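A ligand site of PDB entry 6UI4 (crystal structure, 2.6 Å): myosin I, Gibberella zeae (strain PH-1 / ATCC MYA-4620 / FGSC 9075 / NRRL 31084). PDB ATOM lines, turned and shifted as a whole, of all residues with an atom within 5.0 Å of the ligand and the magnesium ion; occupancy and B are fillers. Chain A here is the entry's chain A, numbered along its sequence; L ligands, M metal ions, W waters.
An oxygen (O6) of the ligand lies close to the backbone carbonyl oxygen (O) of Asn 150, at 3.1 Å. Merely in contact with the ligand: Arg 46, Pro 44, Ala 99, Phe 45, Glu 96, Tyr 373 and Ile 31. Within 4 Å of the ligand: Ile 31, Asn 43, Pro 44, Phe 45, Arg 46, Tyr 51, Glu 96, Ser 97, Gly 98, Ala 99, Gly 100, Lys 101, Thr 102, Glu 103, Asn 148, Asn 150, Ser 151, Ser 152, Tyr 373 and Gly 374. The nearest printed residue that does not touch the ligand is Tyr 32 (4.2 Å).
The backbone NH (N) of Gly 374 sits at hydrogen-bond distance from an oxygen (O2) of the ligand (2.6 Å). An oxygen (O7) of the ligand is in hydrogen-bond range of the backbone NH (N) of Glu 103 (2.8 Å). The side-chain hydroxyl (OG) of Ser 97 sits close to a sulfur (S1) of the ligand, 2.9 Å away. The backbone NH (N) of Lys 101 sits at hydrogen-bond distance from an oxygen (O4) of the ligand, 2.9 Å away. The side-chain amide nitrogen (ND2) of Asn 43 lies within hydrogen-bond range of an oxygen (O10) of the ligand (3.1 Å). The side-chain hydroxyl (OH) of Tyr 51 lies within hydrogen-bond range of a nitrogen (N3) of the ligand (2.8 Å). The side-chain amide nitrogen (ND2) of Asn 148 lies within hydrogen-bond range of an oxygen (O5) of the ligand (2.9 Å). A sulfur (S1) of the ligand sits close to the backbone NH (N) of Ser 152. An oxygen (O4) of the ligand lies within salt-bridge range of the side-chain amino group (NZ) of Lys 101, 2.5 Å away. The backbone NH (N) of Thr 102 lies within hydrogen-bond range of an oxygen (O7) of the ligand. An oxygen (O8) of the ligand is in hydrogen-bond range of the backbone NH (N) of Gly 100, 3.0 Å away. The side-chain hydroxyl (OG) of Ser 151 lies close to a sulfur (S1) of the ligand. The backbone NH (N) of Gly 98 is in hydrogen-bond range of an oxygen (O5) of the ligand (3.0 Å).
NZ of Lys 101 is in hydrogen-bond range of O of Glu 96 (3.3 Å). The side-chain amino group of Lys 101 lies within hydrogen-bond range of the backbone carbonyl oxygen of Gly 95. The side-chain amide oxygen of Asn 148 sits at hydrogen-bond distance from the backbone NH of Asn 150. The side-chain amide oxygen of Asn 150 sits at hydrogen-bond distance from the side-chain amide nitrogen of Asn 142 (3.3 Å). O of Gly 98 is in hydrogen-bond range of ND2 of Asn 43, at 2.6 Å. OH of Tyr 32 lies within hydrogen-bond range of OH of Tyr 51. The side-chain hydroxyl (OG) of Ser 151 is in hydrogen-bond range of the guanidinium group (NH1) of Arg 153, at 3.0 Å. The side-chain hydroxyl (OG1) of Thr 102 lies close to the side-chain carboxylate (OD2) of Asp 371.
Water W1 lies within hydrogen-bond range of OD1 of Asp 371 (2.5 Å) and O of Ile 372 (2.8 Å). Water W2 lies within hydrogen-bond range of an oxygen (O6) of the ligand (2.5 Å), the backbone carbonyl oxygen (O) of Asn 150 (2.5 Å) and the backbone NH (N) of Ser 152 (3.2 Å).
The magnesium ion is bound by water W1 (2.1 Å), water W2 (2.1 Å), an oxygen (O3) of the ligand (2.1 Å), an oxygen (O1) of the ligand (2.1 Å), the side-chain hydroxyl (OG) of Ser 152 (2.1 Å) and the side-chain hydroxyl (OG1) of Thr 102 (2.1 Å).
Asp 371 touches the magnesium ion. Of the 28 residues printed, 3 come within 4 Å of the magnesium ion. The nearest printed residue that does not touch the magnesium ion is Asn 150 (4.5 Å).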
ATOM      1  N   ILE A  31      30.713  24.526  16.766  1.00  0.00           N
ATOM      2  CA  ILE A  31      29.309  24.559  16.350  1.00  0.00           C
ATOM      3  C   ILE A  31      28.998  25.729  15.406  1.00  0.00           C
ATOM      4  O   ILE A  31      27.939  25.735  14.772  1.00  0.00           O
ATOM      5  CB  ILE A  31      28.397  24.602  17.582  1.00  0.00           C
ATOM      6  CG1 ILE A  31      28.501  25.962  18.299  1.00  0.00           C
ATOM      7  CG2 ILE A  31      28.724  23.458  18.521  1.00  0.00           C
ATOM      8  CD1 ILE A  31      27.266  26.332  19.093  1.00  0.00           C
ATOM      9  N   TYR A  32      29.879  26.720  15.315  1.00  0.00           N
ATOM     10  CA  TYR A  32      29.640  27.938  14.533  1.00  0.00           C
ATOM     11  C   TYR A  32      30.463  27.922  13.255  1.00  0.00           C
ATOM     12  O   TYR A  32      31.654  27.601  13.274  1.00  0.00           O
ATOM     13  CB  TYR A  32      29.980  29.173  15.373  1.00  0.00           C
ATOM     14  CG  TYR A  32      29.027  29.449  16.526  1.00  0.00           C
ATOM     15  CD1 TYR A  32      29.489  29.486  17.837  1.00  0.00           C
ATOM     16  CD2 TYR A  32      27.679  29.694  16.301  1.00  0.00           C
ATOM     17  CE1 TYR A  32      28.627  29.731  18.889  1.00  0.00           C
ATOM     18  CE2 TYR A  32      26.807  29.961  17.355  1.00  0.00           C
ATOM     19  CZ  TYR A  32      27.285  29.967  18.655  1.00  0.00           C
ATOM     20  OH  TYR A  32      26.439  30.239  19.700  1.00  0.00           O
ATOM     21  N   ASN A  43      23.375  22.842  16.852  1.00  0.00           N
ATOM     22  CA  ASN A  43      23.031  22.708  18.269  1.00  0.00           C
ATOM     23  C   ASN A  43      23.880  21.630  18.932  1.00  0.00           C
ATOM     24  O   ASN A  43      23.688  20.437  18.650  1.00  0.00           O
ATOM     25  CB  ASN A  43      21.539  22.366  18.415  1.00  0.00           C
ATOM     26  CG  ASN A  43      21.067  22.351  19.866  1.00  0.00           C
ATOM     27  OD1 ASN A  43      21.863  22.318  20.800  1.00  0.00           O
ATOM     28  ND2 ASN A  43      19.750  22.387  20.054  1.00  0.00           N
ATOM     29  N   PRO A  44      24.821  21.996  19.805  1.00  0.00           N
ATOM     30  CA  PRO A  44      25.697  20.978  20.420  1.00  0.00           C
ATOM     31  C   PRO A  44      25.021  20.103  21.464  1.00  0.00           C
ATOM     32  O   PRO A  44      25.540  19.023  21.759  1.00  0.00           O
ATOM     33  CB  PRO A  44      26.812  21.817  21.050  1.00  0.00           C
ATOM     34  CG  PRO A  44      26.131  23.106  21.384  1.00  0.00           C
ATOM     35  CD  PRO A  44      25.155  23.352  20.267  1.00  0.00           C
ATOM     36  N   PHE A  45      23.902  20.552  22.039  1.00  0.00           N
ATOM     37  CA  PHE A  45      23.190  19.828  23.110  1.00  0.00           C
ATOM     38  C   PHE A  45      24.116  19.526  24.278  1.00  0.00           C
ATOM     39  O   PHE A  45      23.943  18.531  24.993  1.00  0.00           O
ATOM     40  CB  PHE A  45      22.549  18.544  22.581  1.00  0.00           C
ATOM     41  CG  PHE A  45      21.305  18.772  21.752  1.00  0.00           C
ATOM     42  CD1 PHE A  45      21.318  18.530  20.390  1.00  0.00           C
ATOM     43  CD2 PHE A  45      20.138  19.221  22.340  1.00  0.00           C
ATOM     44  CE1 PHE A  45      20.176  18.735  19.625  1.00  0.00           C
ATOM     45  CE2 PHE A  45      18.995  19.426  21.575  1.00  0.00           C
ATOM     46  CZ  PHE A  45      19.020  19.183  20.222  1.00  0.00           C
ATOM     47  N   ARG A  46      25.131  20.370  24.486  1.00  0.00           N
ATOM     48  CA  ARG A  46      26.110  20.203  25.540  1.00  0.00           C
ATOM     49  C   ARG A  46      26.704  21.570  25.881  1.00  0.00           C
ATOM     50  O   ARG A  46      26.874  22.400  24.996  1.00  0.00           O
ATOM     51  CB  ARG A  46      27.198  19.219  25.097  1.00  0.00           C
ATOM     52  CG  ARG A  46      28.487  19.230  25.877  1.00  0.00           C
ATOM     53  CD  ARG A  46      29.482  18.204  25.320  1.00  0.00           C
ATOM     54  NE  ARG A  46      29.629  18.322  23.872  1.00  0.00           N
ATOM     55  CZ  ARG A  46      30.564  17.685  23.163  1.00  0.00           C
ATOM     56  NH1 ARG A  46      31.441  16.893  23.771  1.00  0.00           N
ATOM     57  NH2 ARG A  46      30.636  17.841  21.843  1.00  0.00           N
ATOM     58  N   ASP A  47      27.036  21.777  27.156  1.00  0.00           N
ATOM     59  CA  ASP A  47      27.696  23.026  27.548  1.00  0.00           C
ATOM     60  C   ASP A  47      29.167  22.926  27.166  1.00  0.00           C
ATOM     61  O   ASP A  47      29.922  22.146  27.755  1.00  0.00           O
ATOM     62  CB  ASP A  47      27.526  23.310  29.046  1.00  0.00           C
ATOM     63  CG  ASP A  47      28.215  24.608  29.476  1.00  0.00           C
ATOM     64  OD1 ASP A  47      28.551  25.440  28.613  1.00  0.00           O
ATOM     65  OD2 ASP A  47      28.411  24.801  30.702  1.00  0.00           O
ATOM     66  N   TYR A  51      30.646  30.760  26.142  1.00  0.00           N
ATOM     67  CA  TYR A  51      29.912  31.997  26.367  1.00  0.00           C
ATOM     68  C   TYR A  51      30.372  32.673  27.653  1.00  0.00           C
ATOM     69  O   TYR A  51      29.604  33.388  28.313  1.00  0.00           O
ATOM     70  CB  TYR A  51      28.402  31.768  26.358  1.00  0.00           C
ATOM     71  CG  TYR A  51      27.916  31.017  25.139  1.00  0.00           C
ATOM     72  CD1 TYR A  51      27.571  29.673  25.200  1.00  0.00           C
ATOM     73  CD2 TYR A  51      27.845  31.647  23.901  1.00  0.00           C
ATOM     74  CE1 TYR A  51      27.142  28.980  24.085  1.00  0.00           C
ATOM     75  CE2 TYR A  51      27.410  30.963  22.772  1.00  0.00           C
ATOM     76  CZ  TYR A  51      27.061  29.634  22.873  1.00  0.00           C
ATOM     77  OH  TYR A  51      26.642  28.956  21.748  1.00  0.00           O
ATOM     78  N   GLY A  95      15.342  28.145  12.345  1.00  0.00           N
ATOM     79  CA  GLY A  95      15.640  26.859  12.938  1.00  0.00           C
ATOM     80  C   GLY A  95      14.420  26.016  13.231  1.00  0.00           C
ATOM     81  O   GLY A  95      13.376  26.536  13.614  1.00  0.00           O
ATOM     82  N   GLU A  96      14.536  24.698  13.041  1.00  0.00           N
ATOM     83  CA  GLU A  96      13.516  23.787  13.508  1.00  0.00           C
ATOM     84  C   GLU A  96      13.424  23.818  15.029  1.00  0.00           C
ATOM     85  O   GLU A  96      14.336  24.260  15.724  1.00  0.00           O
ATOM     86  CB  GLU A  96      13.820  22.359  13.047  1.00  0.00           C
ATOM     87  CG  GLU A  96      13.871  22.207  11.550  1.00  0.00           C
ATOM     88  CD  GLU A  96      14.218  20.792  11.128  1.00  0.00           C
ATOM     89  OE1 GLU A  96      14.280  19.900  12.004  1.00  0.00           O
ATOM     90  OE2 GLU A  96      14.444  20.577   9.913  1.00  0.00           O
ATOM     91  N   SER A  97      12.279  23.373  15.543  1.00  0.00           N
ATOM     92  CA  SER A  97      12.084  23.252  16.982  1.00  0.00           C
ATOM     93  C   SER A  97      13.211  22.448  17.609  1.00  0.00           C
ATOM     94  O   SER A  97      13.422  21.274  17.277  1.00  0.00           O
ATOM     95  CB  SER A  97      10.729  22.589  17.270  1.00  0.00           C
ATOM     96  OG  SER A  97      10.569  22.295  18.647  1.00  0.00           O
ATOM     97  N   GLY A  98      13.933  23.089  18.521  1.00  0.00           N
ATOM     98  CA  GLY A  98      15.058  22.473  19.205  1.00  0.00           C
ATOM     99  C   GLY A  98      16.414  22.702  18.568  1.00  0.00           C
ATOM    100  O   GLY A  98      17.401  22.097  19.009  1.00  0.00           O
ATOM    101  N   ALA A  99      16.503  23.564  17.551  1.00  0.00           N
ATOM    102  CA  ALA A  99      17.764  23.829  16.876  1.00  0.00           C
ATOM    103  C   ALA A  99      18.631  24.826  17.644  1.00  0.00           C
ATOM    104  O   ALA A  99      19.838  24.877  17.420  1.00  0.00           O
ATOM    105  CB  ALA A  99      17.526  24.331  15.447  1.00  0.00           C
ATOM    106  N   GLY A 100      18.015  25.626  18.519  1.00  0.00           N
ATOM    107  CA  GLY A 100      18.738  26.548  19.363  1.00  0.00           C
ATOM    108  C   GLY A 100      18.546  28.018  19.030  1.00  0.00           C
ATOM    109  O   GLY A 100      19.437  28.836  19.284  1.00  0.00           O
ATOM    110  N   LYS A 101      17.383  28.373  18.472  1.00  0.00           N
ATOM    111  CA  LYS A 101      17.085  29.770  18.192  1.00  0.00           C
ATOM    112  C   LYS A 101      17.091  30.588  19.474  1.00  0.00           C
ATOM    113  O   LYS A 101      17.691  31.668  19.553  1.00  0.00           O
ATOM    114  CB  LYS A 101      15.735  29.892  17.489  1.00  0.00           C
ATOM    115  CG  LYS A 101      15.755  29.539  16.008  1.00  0.00           C
ATOM    116  CD  LYS A 101      14.345  29.515  15.438  1.00  0.00           C
ATOM    117  CE  LYS A 101      13.388  28.828  16.408  1.00  0.00           C
ATOM    118  NZ  LYS A 101      13.653  27.369  16.522  1.00  0.00           N
ATOM    119  N   THR A 102      16.409  30.081  20.512  1.00  0.00           N
ATOM    120  CA  THR A 102      16.212  30.853  21.734  1.00  0.00           C
ATOM    121  C   THR A 102      17.544  31.081  22.454  1.00  0.00           C
ATOM    122  O   THR A 102      17.814  32.184  22.943  1.00  0.00           O
ATOM    123  CB  THR A 102      15.199  30.129  22.635  1.00  0.00           C
ATOM    124  OG1 THR A 102      13.873  30.280  22.083  1.00  0.00           O
ATOM    125  CG2 THR A 102      15.218  30.691  24.038  1.00  0.00           C
ATOM    126  N   GLU A 103      18.398  30.053  22.496  1.00  0.00           N
ATOM    127  CA  GLU A 103      19.695  30.183  23.136  1.00  0.00           C
ATOM    128  C   GLU A 103      20.584  31.189  22.395  1.00  0.00           C
ATOM    129  O   GLU A 103      21.307  31.967  23.022  1.00  0.00           O
ATOM    130  CB  GLU A 103      20.374  28.818  23.218  1.00  0.00           C
ATOM    131  CG  GLU A 103      19.827  27.907  24.313  1.00  0.00           C
ATOM    132  CD  GLU A 103      19.803  28.568  25.680  1.00  0.00           C
ATOM    133  OE1 GLU A 103      20.766  29.298  26.015  1.00  0.00           O
ATOM    134  OE2 GLU A 103      18.826  28.347  26.429  1.00  0.00           O
ATOM    135  N   ASN A 142       7.347  28.771  27.817  1.00  0.00           N
ATOM    136  CA  ASN A 142       8.071  27.583  27.388  1.00  0.00           C
ATOM    137  C   ASN A 142       7.574  26.355  28.155  1.00  0.00           C
ATOM    138  O   ASN A 142       7.093  26.461  29.286  1.00  0.00           O
ATOM    139  CB  ASN A 142       9.582  27.767  27.578  1.00  0.00           C
ATOM    140  CG  ASN A 142      10.154  28.840  26.649  1.00  0.00           C
ATOM    141  OD1 ASN A 142       9.463  29.792  26.280  1.00  0.00           O
ATOM    142  ND2 ASN A 142      11.413  28.682  26.261  1.00  0.00           N
ATOM    143  N   ASN A 148      11.767  19.265  22.114  1.00  0.00           N
ATOM    144  CA  ASN A 148      12.627  20.211  22.818  1.00  0.00           C
ATOM    145  C   ASN A 148      12.139  20.358  24.251  1.00  0.00           C
ATOM    146  O   ASN A 148      10.937  20.562  24.498  1.00  0.00           O
ATOM    147  CB  ASN A 148      12.661  21.566  22.079  1.00  0.00           C
ATOM    148  CG  ASN A 148      13.407  22.654  22.847  1.00  0.00           C
ATOM    149  OD1 ASN A 148      14.115  22.388  23.816  1.00  0.00           O
ATOM    150  ND2 ASN A 148      13.294  23.883  22.370  1.00  0.00           N
ATOM    151  N   ASN A 150      13.026  22.774  26.485  1.00  0.00           N
ATOM    152  CA  ASN A 150      12.714  24.163  26.797  1.00  0.00           C
ATOM    153  C   ASN A 150      12.186  24.834  25.524  1.00  0.00           C
ATOM    154  O   ASN A 150      12.846  25.689  24.930  1.00  0.00           O
ATOM    155  CB  ASN A 150      13.961  24.869  27.353  1.00  0.00           C
ATOM    156  CG  ASN A 150      13.683  26.299  27.760  1.00  0.00           C
ATOM    157  OD1 ASN A 150      12.686  26.572  28.434  1.00  0.00           O
ATOM    158  ND2 ASN A 150      14.548  27.210  27.347  1.00  0.00           N
ATOM    159  N   SER A 151      10.980  24.428  25.132  1.00  0.00           N
ATOM    160  CA  SER A 151      10.405  24.757  23.833  1.00  0.00           C
ATOM    161  C   SER A 151       9.593  26.050  23.902  1.00  0.00           C
ATOM    162  O   SER A 151       8.595  26.115  24.632  1.00  0.00           O
ATOM    163  CB  SER A 151       9.527  23.607  23.337  1.00  0.00           C
ATOM    164  OG  SER A 151       8.734  24.014  22.230  1.00  0.00           O
ATOM    165  N   SER A 152      10.019  27.070  23.164  1.00  0.00           N
ATOM    166  CA  SER A 152       9.237  28.287  23.045  1.00  0.00           C
ATOM    167  C   SER A 152       7.855  27.986  22.454  1.00  0.00           C
ATOM    168  O   SER A 152       7.761  27.469  21.334  1.00  0.00           O
ATOM    169  CB  SER A 152       9.980  29.298  22.169  1.00  0.00           C
ATOM    170  OG  SER A 152      11.317  29.499  22.626  1.00  0.00           O
ATOM    171  N   ARG A 153       6.785  28.277  23.207  1.00  0.00           N
ATOM    172  CA  ARG A 153       5.432  28.085  22.727  1.00  0.00           C
ATOM    173  C   ARG A 153       4.770  29.404  22.365  1.00  0.00           C
ATOM    174  O   ARG A 153       3.540  29.486  22.256  1.00  0.00           O
ATOM    175  CB  ARG A 153       4.564  27.356  23.763  1.00  0.00           C
ATOM    176  CG  ARG A 153       5.110  26.049  24.298  1.00  0.00           C
ATOM    177  CD  ARG A 153       5.635  25.111  23.229  1.00  0.00           C
ATOM    178  NE  ARG A 153       4.618  24.694  22.264  1.00  0.00           N
ATOM    179  CZ  ARG A 153       4.908  24.130  21.098  1.00  0.00           C
ATOM    180  NH1 ARG A 153       6.172  23.888  20.773  1.00  0.00           N
ATOM    181  NH2 ARG A 153       3.945  23.786  20.255  1.00  0.00           N
ATOM    182  N   ASP A 371      12.890  35.865  17.931  1.00  0.00           N
ATOM    183  CA  ASP A 371      12.895  34.484  18.443  1.00  0.00           C
ATOM    184  C   ASP A 371      11.486  33.900  18.305  1.00  0.00           C
ATOM    185  O   ASP A 371      10.662  34.010  19.230  1.00  0.00           O
ATOM    186  CB  ASP A 371      13.402  34.431  19.888  1.00  0.00           C
ATOM    187  CG  ASP A 371      13.324  33.016  20.473  1.00  0.00           C
ATOM    188  OD1 ASP A 371      13.523  32.045  19.714  1.00  0.00           O
ATOM    189  OD2 ASP A 371      13.099  32.893  21.693  1.00  0.00           O
ATOM    190  N   ILE A 372      11.199  33.318  17.144  1.00  0.00           N
ATOM    191  CA  ILE A 372       9.936  32.621  16.875  1.00  0.00           C
ATOM    192  C   ILE A 372      10.019  31.173  17.341  1.00  0.00           C
ATOM    193  O   ILE A 372      11.105  30.661  17.629  1.00  0.00           O
ATOM    194  CB  ILE A 372       9.565  32.681  15.389  1.00  0.00           C
ATOM    195  CG1 ILE A 372      10.500  31.754  14.593  1.00  0.00           C
ATOM    196  CG2 ILE A 372       9.618  34.099  14.866  1.00  0.00           C
ATOM    197  CD1 ILE A 372      10.263  31.783  13.108  1.00  0.00           C
ATOM    198  N   TYR A 373       8.879  30.500  17.392  1.00  0.00           N
ATOM    199  CA  TYR A 373       8.843  29.055  17.603  1.00  0.00           C
ATOM    200  C   TYR A 373       9.186  28.361  16.292  1.00  0.00           C
ATOM    201  O   TYR A 373       8.644  28.719  15.233  1.00  0.00           O
ATOM    202  CB  TYR A 373       7.483  28.587  18.140  1.00  0.00           C
ATOM    203  CG  TYR A 373       6.266  29.478  17.908  1.00  0.00           C
ATOM    204  CD1 TYR A 373       6.144  30.277  16.773  1.00  0.00           C
ATOM    205  CD2 TYR A 373       5.243  29.533  18.844  1.00  0.00           C
ATOM    206  CE1 TYR A 373       5.044  31.093  16.580  1.00  0.00           C
ATOM    207  CE2 TYR A 373       4.129  30.346  18.656  1.00  0.00           C
ATOM    208  CZ  TYR A 373       4.041  31.125  17.522  1.00  0.00           C
ATOM    209  OH  TYR A 373       2.944  31.926  17.312  1.00  0.00           O
ATOM    210  N   GLY A 374      10.080  27.377  16.359  1.00  0.00           N
ATOM    211  CA  GLY A 374      10.588  26.708  15.163  1.00  0.00           C
ATOM    212  C   GLY A 374       9.608  25.745  14.523  1.00  0.00           C
ATOM    213  O   GLY A 374       8.622  25.310  15.104  1.00  0.00           O
ATOM    214  N   GLU A 376       7.880  22.530  13.328  1.00  0.00           N
ATOM    215  CA  GLU A 376       7.738  21.285  14.088  1.00  0.00           C
ATOM    216  C   GLU A 376       6.626  20.415  13.518  1.00  0.00           C
ATOM    217  O   GLU A 376       5.727  20.882  12.811  1.00  0.00           O
ATOM    218  CB  GLU A 376       7.452  21.588  15.562  1.00  0.00           C
ATOM    219  CG  GLU A 376       6.157  22.342  15.807  1.00  0.00           C
ATOM    220  CD  GLU A 376       6.002  22.798  17.252  1.00  0.00           C
ATOM    221  OE1 GLU A 376       6.973  23.345  17.811  1.00  0.00           O
ATOM    222  OE2 GLU A 376       4.905  22.601  17.816  1.00  0.00           O
HETATM  223  P1  LIG L   1      11.787  26.137  19.651  1.00  0.00           P
HETATM  224  S1  LIG L   1      10.503  24.808  20.176  1.00  0.00           S
HETATM  225  O1  LIG L   1      11.449  27.431  20.371  1.00  0.00           O
HETATM  226  O2  LIG L   1      11.701  26.372  18.152  1.00  0.00           O
HETATM  227  P2  LIG L   1      14.656  26.500  19.914  1.00  0.00           P
HETATM  228  O3  LIG L   1      14.491  27.873  20.491  1.00  0.00           O
HETATM  229  O4  LIG L   1      15.065  26.638  18.443  1.00  0.00           O
HETATM  230  O5  LIG L   1      13.301  25.600  20.031  1.00  0.00           O
HETATM  231  P3  LIG L   1      16.490  26.219  22.167  1.00  0.00           P
HETATM  232  O6  LIG L   1      15.353  26.322  23.167  1.00  0.00           O
HETATM  233  O7  LIG L   1      17.189  27.559  22.035  1.00  0.00           O
HETATM  234  O8  LIG L   1      15.894  25.729  20.700  1.00  0.00           O
HETATM  235  O9  LIG L   1      17.584  25.070  22.672  1.00  0.00           O
HETATM  236  C1  LIG L   1      17.102  23.759  22.835  1.00  0.00           C
HETATM  237  C2  LIG L   1      18.086  23.045  23.788  1.00  0.00           C
HETATM  238  O10 LIG L   1      19.168  22.719  23.117  1.00  0.00           O
HETATM  239  C3  LIG L   1      18.581  24.050  24.904  1.00  0.00           C
HETATM  240  O11 LIG L   1      17.804  23.943  26.001  1.00  0.00           O
HETATM  241  C4  LIG L   1      20.014  23.585  25.191  1.00  0.00           C
HETATM  242  O12 LIG L   1      19.994  22.431  26.103  1.00  0.00           O
HETATM  243  C5  LIG L   1      20.478  23.187  24.012  1.00  0.00           C
HETATM  244  N1  LIG L   1      21.191  24.216  23.341  1.00  0.00           N
HETATM  245  C6  LIG L   1      20.731  25.014  22.389  1.00  0.00           C
HETATM  246  N2  LIG L   1      21.707  25.841  21.998  1.00  0.00           N
HETATM  247  C7  LIG L   1      22.807  25.565  22.718  1.00  0.00           C
HETATM  248  C8  LIG L   1      24.126  26.093  22.746  1.00  0.00           C
HETATM  249  N3  LIG L   1      24.521  27.169  21.874  1.00  0.00           N
HETATM  250  N4  LIG L   1      24.988  25.556  23.599  1.00  0.00           N
HETATM  251  C9  LIG L   1      24.648  24.564  24.403  1.00  0.00           C
HETATM  252  N5  LIG L   1      23.428  24.044  24.402  1.00  0.00           N
HETATM  253  C10 LIG L   1      22.487  24.531  23.560  1.00  0.00           C
HETATM  254 MG    MG M   1      12.799  28.561  21.482  1.00  0.00          MG
HETATM  255  O   HOH W   1      12.289  29.951  20.038  1.00  0.00           O
HETATM  256  O   HOH W   2      13.167  27.529  23.248  1.00  0.00           O
HETATM  257  O   HOH W   3       8.494  25.222  17.894  1.00  0.00           O
HETATM  258  O   HOH W   4      23.008  22.992  27.466  1.00  0.00           O
